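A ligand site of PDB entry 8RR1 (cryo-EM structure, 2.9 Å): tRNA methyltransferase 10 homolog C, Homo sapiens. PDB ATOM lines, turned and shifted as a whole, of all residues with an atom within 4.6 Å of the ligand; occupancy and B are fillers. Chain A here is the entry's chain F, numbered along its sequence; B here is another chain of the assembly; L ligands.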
ATOM      1  N   LEU A 202      10.348  12.404 -19.021  1.00  0.00           N
ATOM      2  CA  LEU A 202      10.593  13.295 -17.899  1.00  0.00           C
ATOM      3  C   LEU A 202      11.052  12.491 -16.682  1.00  0.00           C
ATOM      4  O   LEU A 202      10.443  11.481 -16.321  1.00  0.00           O
ATOM      5  CB  LEU A 202       9.322  14.076 -17.559  1.00  0.00           C
ATOM      6  CG  LEU A 202       8.912  15.167 -18.545  1.00  0.00           C
ATOM      7  CD1 LEU A 202       7.518  15.680 -18.228  1.00  0.00           C
ATOM      8  CD2 LEU A 202       9.910  16.308 -18.530  1.00  0.00           C
ATOM      9  N   THR A 203      12.143  12.937 -16.067  1.00  0.00           N
ATOM     10  CA  THR A 203      12.642  12.310 -14.846  1.00  0.00           C
ATOM     11  C   THR A 203      13.503  13.325 -14.103  1.00  0.00           C
ATOM     12  O   THR A 203      14.048  14.255 -14.695  1.00  0.00           O
ATOM     13  CB  THR A 203      13.436  11.032 -15.144  1.00  0.00           C
ATOM     14  OG1 THR A 203      13.650  10.309 -13.932  1.00  0.00           O
ATOM     15  CG2 THR A 203      14.771  11.360 -15.780  1.00  0.00           C
ATOM     16  N   ALA A 204      13.598  13.129 -12.782  1.00  0.00           N
ATOM     17  CA  ALA A 204      14.382  14.032 -11.957  1.00  0.00           C
ATOM     18  C   ALA A 204      15.882  13.788 -12.057  1.00  0.00           C
ATOM     19  O   ALA A 204      16.668  14.669 -11.697  1.00  0.00           O
ATOM     20  CB  ALA A 204      13.938  13.920 -10.497  1.00  0.00           C
ATOM     21  N   ASP A 205      16.291  12.612 -12.522  1.00  0.00           N
ATOM     22  CA  ASP A 205      17.697  12.255 -12.608  1.00  0.00           C
ATOM     23  C   ASP A 205      18.320  12.567 -13.969  1.00  0.00           C
ATOM     24  O   ASP A 205      19.489  12.254 -14.187  1.00  0.00           O
ATOM     25  CB  ASP A 205      17.887  10.770 -12.285  1.00  0.00           C
ATOM     26  CG  ASP A 205      17.286  10.383 -10.957  1.00  0.00           C
ATOM     27  OD1 ASP A 205      17.448  11.150  -9.984  1.00  0.00           O
ATOM     28  OD2 ASP A 205      16.640   9.313 -10.878  1.00  0.00           O
ATOM     29  N   VAL A 220       6.509  11.700 -21.431  1.00  0.00           N
ATOM     30  CA  VAL A 220       6.178  10.471 -20.708  1.00  0.00           C
ATOM     31  C   VAL A 220       6.418  10.706 -19.231  1.00  0.00           C
ATOM     32  O   VAL A 220       7.510  11.132 -18.819  1.00  0.00           O
ATOM     33  CB  VAL A 220       7.004   9.276 -21.218  1.00  0.00           C
ATOM     34  CG1 VAL A 220       6.584   7.997 -20.519  1.00  0.00           C
ATOM     35  CG2 VAL A 220       6.870   9.140 -22.724  1.00  0.00           C
ATOM     36  N   ILE A 221       5.399  10.444 -18.419  1.00  0.00           N
ATOM     37  CA  ILE A 221       5.479  10.559 -16.965  1.00  0.00           C
ATOM     38  C   ILE A 221       5.330   9.167 -16.373  1.00  0.00           C
ATOM     39  O   ILE A 221       4.329   8.491 -16.624  1.00  0.00           O
ATOM     40  CB  ILE A 221       4.410  11.513 -16.417  1.00  0.00           C
ATOM     41  CG1 ILE A 221       4.599  12.914 -16.990  1.00  0.00           C
ATOM     42  CG2 ILE A 221       4.479  11.556 -14.893  1.00  0.00           C
ATOM     43  CD1 ILE A 221       3.480  13.872 -16.638  1.00  0.00           C
ATOM     44  N   GLY A 222       6.323   8.737 -15.608  1.00  0.00           N
ATOM     45  CA  GLY A 222       6.292   7.420 -15.012  1.00  0.00           C
ATOM     46  C   GLY A 222       5.288   7.371 -13.876  1.00  0.00           C
ATOM     47  O   GLY A 222       5.421   8.115 -12.883  1.00  0.00           O
ATOM     48  N   PHE A 224       4.666   6.323 -10.963  1.00  0.00           N
ATOM     49  CA  PHE A 224       5.491   5.754  -9.908  1.00  0.00           C
ATOM     50  C   PHE A 224       5.280   6.577  -8.645  1.00  0.00           C
ATOM     51  O   PHE A 224       4.934   7.759  -8.708  1.00  0.00           O
ATOM     52  CB  PHE A 224       6.964   5.751 -10.322  1.00  0.00           C
ATOM     53  CG  PHE A 224       7.806   4.739  -9.596  1.00  0.00           C
ATOM     54  CD1 PHE A 224       7.224   3.688  -8.914  1.00  0.00           C
ATOM     55  CD2 PHE A 224       9.190   4.830  -9.626  1.00  0.00           C
ATOM     56  CE1 PHE A 224       8.010   2.752  -8.258  1.00  0.00           C
ATOM     57  CE2 PHE A 224       9.977   3.902  -8.965  1.00  0.00           C
ATOM     58  CZ  PHE A 224       9.387   2.863  -8.281  1.00  0.00           C
ATOM     59  N   VAL A 225       5.476   5.946  -7.496  1.00  0.00           N
ATOM     60  CA  VAL A 225       5.400   6.652  -6.217  1.00  0.00           C
ATOM     61  C   VAL A 225       6.781   6.608  -5.571  1.00  0.00           C
ATOM     62  O   VAL A 225       7.378   7.650  -5.303  1.00  0.00           O
ATOM     63  CB  VAL A 225       4.319   6.059  -5.306  1.00  0.00           C
ATOM     64  CG1 VAL A 225       4.619   6.374  -3.846  1.00  0.00           C
ATOM     65  CG2 VAL A 225       2.957   6.609  -5.682  1.00  0.00           C
ATOM     66  N   ASP A 226       7.288   5.397  -5.321  1.00  0.00           N
ATOM     67  CA  ASP A 226       8.651   5.191  -4.845  1.00  0.00           C
ATOM     68  C   ASP A 226       8.899   5.921  -3.524  1.00  0.00           C
ATOM     69  O   ASP A 226       9.718   6.832  -3.423  1.00  0.00           O
ATOM     70  CB  ASP A 226       9.668   5.615  -5.910  1.00  0.00           C
ATOM     71  CG  ASP A 226      11.085   5.255  -5.551  1.00  0.00           C
ATOM     72  OD1 ASP A 226      11.272   4.241  -4.832  1.00  0.00           O
ATOM     73  OD2 ASP A 226      12.019   5.965  -5.981  1.00  0.00           O
ATOM     74  N   THR A 233      15.316   4.615 -11.431  1.00  0.00           N
ATOM     75  CA  THR A 233      14.499   3.613 -12.109  1.00  0.00           C
ATOM     76  C   THR A 233      13.958   4.137 -13.425  1.00  0.00           C
ATOM     77  O   THR A 233      14.075   3.483 -14.465  1.00  0.00           O
ATOM     78  CB  THR A 233      13.353   3.164 -11.190  1.00  0.00           C
ATOM     79  OG1 THR A 233      13.898   2.535 -10.022  1.00  0.00           O
ATOM     80  CG2 THR A 233      12.448   2.178 -11.917  1.00  0.00           C
ATOM     81  N   SER A 234      13.341   5.321 -13.395  1.00  0.00           N
ATOM     82  CA  SER A 234      12.821   5.917 -14.623  1.00  0.00           C
ATOM     83  C   SER A 234      13.951   6.249 -15.601  1.00  0.00           C
ATOM     84  O   SER A 234      13.801   6.072 -16.816  1.00  0.00           O
ATOM     85  CB  SER A 234      12.016   7.173 -14.292  1.00  0.00           C
ATOM     86  OG  SER A 234      12.823   8.149 -13.665  1.00  0.00           O
ATOM     87  N   GLU A 246      14.606  14.584 -19.757  1.00  0.00           N
ATOM     88  CA  GLU A 246      14.621  15.971 -19.320  1.00  0.00           C
ATOM     89  C   GLU A 246      14.222  16.049 -17.857  1.00  0.00           C
ATOM     90  O   GLU A 246      13.572  15.140 -17.322  1.00  0.00           O
ATOM     91  CB  GLU A 246      13.676  16.842 -20.166  1.00  0.00           C
ATOM     92  CG  GLU A 246      14.271  17.335 -21.471  1.00  0.00           C
ATOM     93  CD  GLU A 246      13.577  18.572 -22.007  1.00  0.00           C
ATOM     94  OE1 GLU A 246      12.404  18.797 -21.644  1.00  0.00           O
ATOM     95  OE2 GLU A 246      14.196  19.315 -22.793  1.00  0.00           O
ATOM     96  N   CYS A 247      14.627  17.129 -17.202  1.00  0.00           N
ATOM     97  CA  CYS A 247      14.270  17.388 -15.813  1.00  0.00           C
ATOM     98  C   CYS A 247      13.782  18.825 -15.685  1.00  0.00           C
ATOM     99  O   CYS A 247      14.250  19.727 -16.388  1.00  0.00           O
ATOM    100  CB  CYS A 247      15.457  17.140 -14.869  1.00  0.00           C
ATOM    101  SG  CYS A 247      16.778  18.367 -14.991  1.00  0.00           S
ATOM    102  N   LEU A 248      12.832  19.026 -14.776  1.00  0.00           N
ATOM    103  CA  LEU A 248      12.303  20.358 -14.564  1.00  0.00           C
ATOM    104  C   LEU A 248      13.378  21.266 -13.949  1.00  0.00           C
ATOM    105  O   LEU A 248      14.122  20.833 -13.068  1.00  0.00           O
ATOM    106  CB  LEU A 248      11.083  20.312 -13.641  1.00  0.00           C
ATOM    107  CG  LEU A 248       9.845  19.591 -14.176  1.00  0.00           C
ATOM    108  CD1 LEU A 248       8.688  19.741 -13.208  1.00  0.00           C
ATOM    109  CD2 LEU A 248       9.463  20.133 -15.551  1.00  0.00           C
ATOM    110  N   LEU A 250      13.708  23.090 -11.594  1.00  0.00           N
ATOM    111  CA  LEU A 250      13.206  23.548 -10.286  1.00  0.00           C
ATOM    112  C   LEU A 250      14.285  24.444  -9.690  1.00  0.00           C
ATOM    113  O   LEU A 250      13.955  25.546  -9.231  1.00  0.00           O
ATOM    114  CB  LEU A 250      12.943  22.306  -9.442  1.00  0.00           C
ATOM    115  CG  LEU A 250      11.913  21.337 -10.025  1.00  0.00           C
ATOM    116  CD1 LEU A 250      11.656  20.194  -9.060  1.00  0.00           C
ATOM    117  CD2 LEU A 250      10.616  22.063 -10.326  1.00  0.00           C
ATOM    118  N   LYS A 261      13.298  16.118  -4.932  1.00  0.00           N
ATOM    119  CA  LYS A 261      12.813  16.889  -6.065  1.00  0.00           C
ATOM    120  C   LYS A 261      11.788  16.132  -6.903  1.00  0.00           C
ATOM    121  O   LYS A 261      11.241  16.714  -7.844  1.00  0.00           O
ATOM    122  CB  LYS A 261      13.993  17.313  -6.950  1.00  0.00           C
ATOM    123  CG  LYS A 261      14.807  18.450  -6.364  1.00  0.00           C
ATOM    124  CD  LYS A 261      16.061  18.730  -7.169  1.00  0.00           C
ATOM    125  CE  LYS A 261      16.906  19.817  -6.513  1.00  0.00           C
ATOM    126  NZ  LYS A 261      18.229  19.976  -7.184  1.00  0.00           N
ATOM    127  N   ASN A 262      11.519  14.864  -6.588  1.00  0.00           N
ATOM    128  CA  ASN A 262      10.458  14.143  -7.263  1.00  0.00           C
ATOM    129  C   ASN A 262       9.108  14.710  -6.869  1.00  0.00           C
ATOM    130  O   ASN A 262       8.833  14.947  -5.684  1.00  0.00           O
ATOM    131  CB  ASN A 262      10.536  12.655  -6.923  1.00  0.00           C
ATOM    132  CG  ASN A 262      11.846  12.026  -7.330  1.00  0.00           C
ATOM    133  OD1 ASN A 262      12.180  11.980  -8.516  1.00  0.00           O
ATOM    134  ND2 ASN A 262      12.597  11.540  -6.354  1.00  0.00           N
ATOM    135  N   LEU A 263       8.243  14.933  -7.858  1.00  0.00           N
ATOM    136  CA  LEU A 263       6.928  15.509  -7.639  1.00  0.00           C
ATOM    137  C   LEU A 263       5.843  14.479  -7.915  1.00  0.00           C
ATOM    138  O   LEU A 263       6.058  13.481  -8.603  1.00  0.00           O
ATOM    139  CB  LEU A 263       6.710  16.740  -8.528  1.00  0.00           C
ATOM    140  CG  LEU A 263       7.759  17.849  -8.418  1.00  0.00           C
ATOM    141  CD1 LEU A 263       7.397  19.014  -9.322  1.00  0.00           C
ATOM    142  CD2 LEU A 263       7.905  18.312  -6.981  1.00  0.00           C
ATOM    143  N   LEU A 265       2.176  13.032  -9.399  1.00  0.00           N
ATOM    144  CA  LEU A 265       1.668  13.018 -10.765  1.00  0.00           C
ATOM    145  C   LEU A 265       0.761  14.217 -11.032  1.00  0.00           C
ATOM    146  O   LEU A 265       0.822  14.818 -12.109  1.00  0.00           O
ATOM    147  CB  LEU A 265       0.930  11.710 -11.039  1.00  0.00           C
ATOM    148  CG  LEU A 265       1.734  10.434 -10.810  1.00  0.00           C
ATOM    149  CD1 LEU A 265       0.924   9.217 -11.211  1.00  0.00           C
ATOM    150  CD2 LEU A 265       3.045  10.477 -11.577  1.00  0.00           C
ATOM    151  N   MET A 268       2.833  17.337 -11.522  1.00  0.00           N
ATOM    152  CA  MET A 268       3.502  17.313 -12.822  1.00  0.00           C
ATOM    153  C   MET A 268       2.537  17.661 -13.950  1.00  0.00           C
ATOM    154  O   MET A 268       2.874  18.447 -14.844  1.00  0.00           O
ATOM    155  CB  MET A 268       4.136  15.947 -13.066  1.00  0.00           C
ATOM    156  CG  MET A 268       5.368  15.675 -12.216  1.00  0.00           C
ATOM    157  SD  MET A 268       6.853  16.463 -12.865  1.00  0.00           S
ATOM    158  CE  MET A 268       6.591  16.294 -14.629  1.00  0.00           C
ATOM    159  P     G B   9       3.602  12.008   2.443  1.00  0.00           P
ATOM    160  OP1   G B   9       2.365  11.189   2.529  1.00  0.00           O
ATOM    161  OP2   G B   9       4.914  11.371   2.757  1.00  0.00           O
ATOM    162  O5'   G B   9       3.689  12.619   0.979  1.00  0.00           O
ATOM    163  C5'   G B   9       2.624  13.388   0.451  1.00  0.00           C
ATOM    164  C4'   G B   9       2.139  12.858  -0.874  1.00  0.00           C
ATOM    165  O4'   G B   9       3.234  12.846  -1.824  1.00  0.00           O
ATOM    166  C3'   G B   9       1.581  11.437  -0.840  1.00  0.00           C
ATOM    167  O3'   G B   9       0.538  11.319  -1.813  1.00  0.00           O
ATOM    168  C2'   G B   9       2.774  10.610  -1.302  1.00  0.00           C
ATOM    169  O2'   G B   9       2.448   9.350  -1.842  1.00  0.00           O
ATOM    170  C1'   G B   9       3.388  11.531  -2.347  1.00  0.00           C
ATOM    171  N9    G B   9       4.806  11.299  -2.617  1.00  0.00           N
ATOM    172  C8    G B   9       5.846  11.359  -1.737  1.00  0.00           C
ATOM    173  N7    G B   9       6.997  11.104  -2.285  1.00  0.00           N
ATOM    174  C5    G B   9       6.700  10.858  -3.616  1.00  0.00           C
ATOM    175  C6    G B   9       7.536  10.526  -4.714  1.00  0.00           C
ATOM    176  O6    G B   9       8.763  10.370  -4.723  1.00  0.00           O
ATOM    177  N1    G B   9       6.808  10.367  -5.884  1.00  0.00           N
ATOM    178  C2    G B   9       5.448  10.509  -6.002  1.00  0.00           C
ATOM    179  N2    G B   9       4.932  10.308  -7.220  1.00  0.00           N
ATOM    180  N3    G B   9       4.652  10.821  -4.986  1.00  0.00           N
ATOM    181  C4    G B   9       5.344  10.976  -3.842  1.00  0.00           C
HETATM  182  N1  LIG L   1      11.415   6.741  -9.270  1.00  0.00           N
HETATM  183  C1  LIG L   1      10.974   8.072  -9.753  1.00  0.00           C
HETATM  184  C2  LIG L   1      10.098   8.761  -8.712  1.00  0.00           C
HETATM  185  C3  LIG L   1       9.339   9.966  -9.231  1.00  0.00           C
HETATM  186  S1  LIG L   1       7.609   9.609  -9.579  1.00  0.00           S
HETATM  187  C4  LIG L   1      12.241   8.895 -10.007  1.00  0.00           C
HETATM  188  O1  LIG L   1      12.799   9.382  -9.015  1.00  0.00           O
HETATM  189  O2  LIG L   1      12.633   8.967 -11.174  1.00  0.00           O
HETATM  190  C5  LIG L   1       7.027  11.070 -10.470  1.00  0.00           C
HETATM  191  C6  LIG L   1       7.313  11.037 -11.953  1.00  0.00           C
HETATM  192  O3  LIG L   1       7.068  12.344 -12.509  1.00  0.00           O
HETATM  193  C7  LIG L   1       8.755  10.690 -12.322  1.00  0.00           C
HETATM  194  O4  LIG L   1       8.886   9.301 -12.593  1.00  0.00           O
HETATM  195  C8  LIG L   1       8.981  11.532 -13.570  1.00  0.00           C
HETATM  196  O5  LIG L   1       8.402  10.921 -14.698  1.00  0.00           O
HETATM  197  C9  LIG L   1       8.224  12.789 -13.192  1.00  0.00           C
HETATM  198  N2  LIG L   1       8.955  13.698 -12.318  1.00  0.00           N
HETATM  199  C10 LIG L   1       8.906  13.762 -10.955  1.00  0.00           C
HETATM  200  N3  LIG L   1       9.675  14.685 -10.442  1.00  0.00           N
HETATM  201  C11 LIG L   1      10.274  15.280 -11.542  1.00  0.00           C
HETATM  202  C12 LIG L   1      11.197  16.328 -11.666  1.00  0.00           C
HETATM  203  N4  LIG L   1      11.696  16.992 -10.627  1.00  0.00           N
HETATM  204  N5  LIG L   1      11.592  16.667 -12.905  1.00  0.00           N
HETATM  205  C13 LIG L   1      11.079  16.001 -13.940  1.00  0.00           C
HETATM  206  N6  LIG L   1      10.212  15.005 -13.950  1.00  0.00           N
HETATM  207  C14 LIG L   1       9.832  14.684 -12.704  1.00  0.00           C
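An oxygen (O2) of the ligand lies within hydrogen-bond range of the side-chain hydroxyl of Ser 234.
N of Leu 248 is in hydrogen-bond range of N5 of the ligand (3.3 Å).
OG1 of Thr 203 lies within hydrogen-bond range of O2 of the ligand (3.2 Å).
The backbone NH (N) of Gly 222 sits at hydrogen-bond distance from an oxygen (O5) of the ligand.
The backbone NH of Leu 263 sits at hydrogen-bond distance from a nitrogen (N3) of the ligand, 3.0 Å away.
N1 of the ligand is in salt-bridge range of OD2 of Asp 226 (3.4 Å).
The backbone carbonyl oxygen of Leu 202 lies within hydrogen-bond range of an oxygen (O5) of the ligand, at 2.7 Å.
An oxygen (O1) of the ligand lies close to the side-chain amide oxygen (OD1) of Asn 262.
A nitrogen (N4) of the ligand is in hydrogen-bond range of the backbone carbonyl oxygen of Lys 261 (2.8 Å).
N of Thr 203 sits at hydrogen-bond distance from O of Glu 246.
O of Val 220 sits at hydrogen-bond distance from N of Leu 202 (3.1 Å).
The backbone carbonyl oxygen (O) of Phe 224 lies close to a sulfur (S1) of the ligand, 3.4 Å away.
The side-chain sulfur of Met 268 lies close to a nitrogen (N2) of the ligand (3.5 Å).
S1 of the ligand lies close to N2 of G 9 of chain B, 3.6 Å away.
Merely in contact with the ligand: Ala 204, Ile 221, Cys 247 and Leu 250.
Hydrophobic or aromatic side chains within 4 Å of the ligand: Leu 202, Ala 204, Ile 221, Phe 224, Leu 248, Leu 250 and Met 268.
Of the 22 residues printed, 16 come within 4 Å of the ligand.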
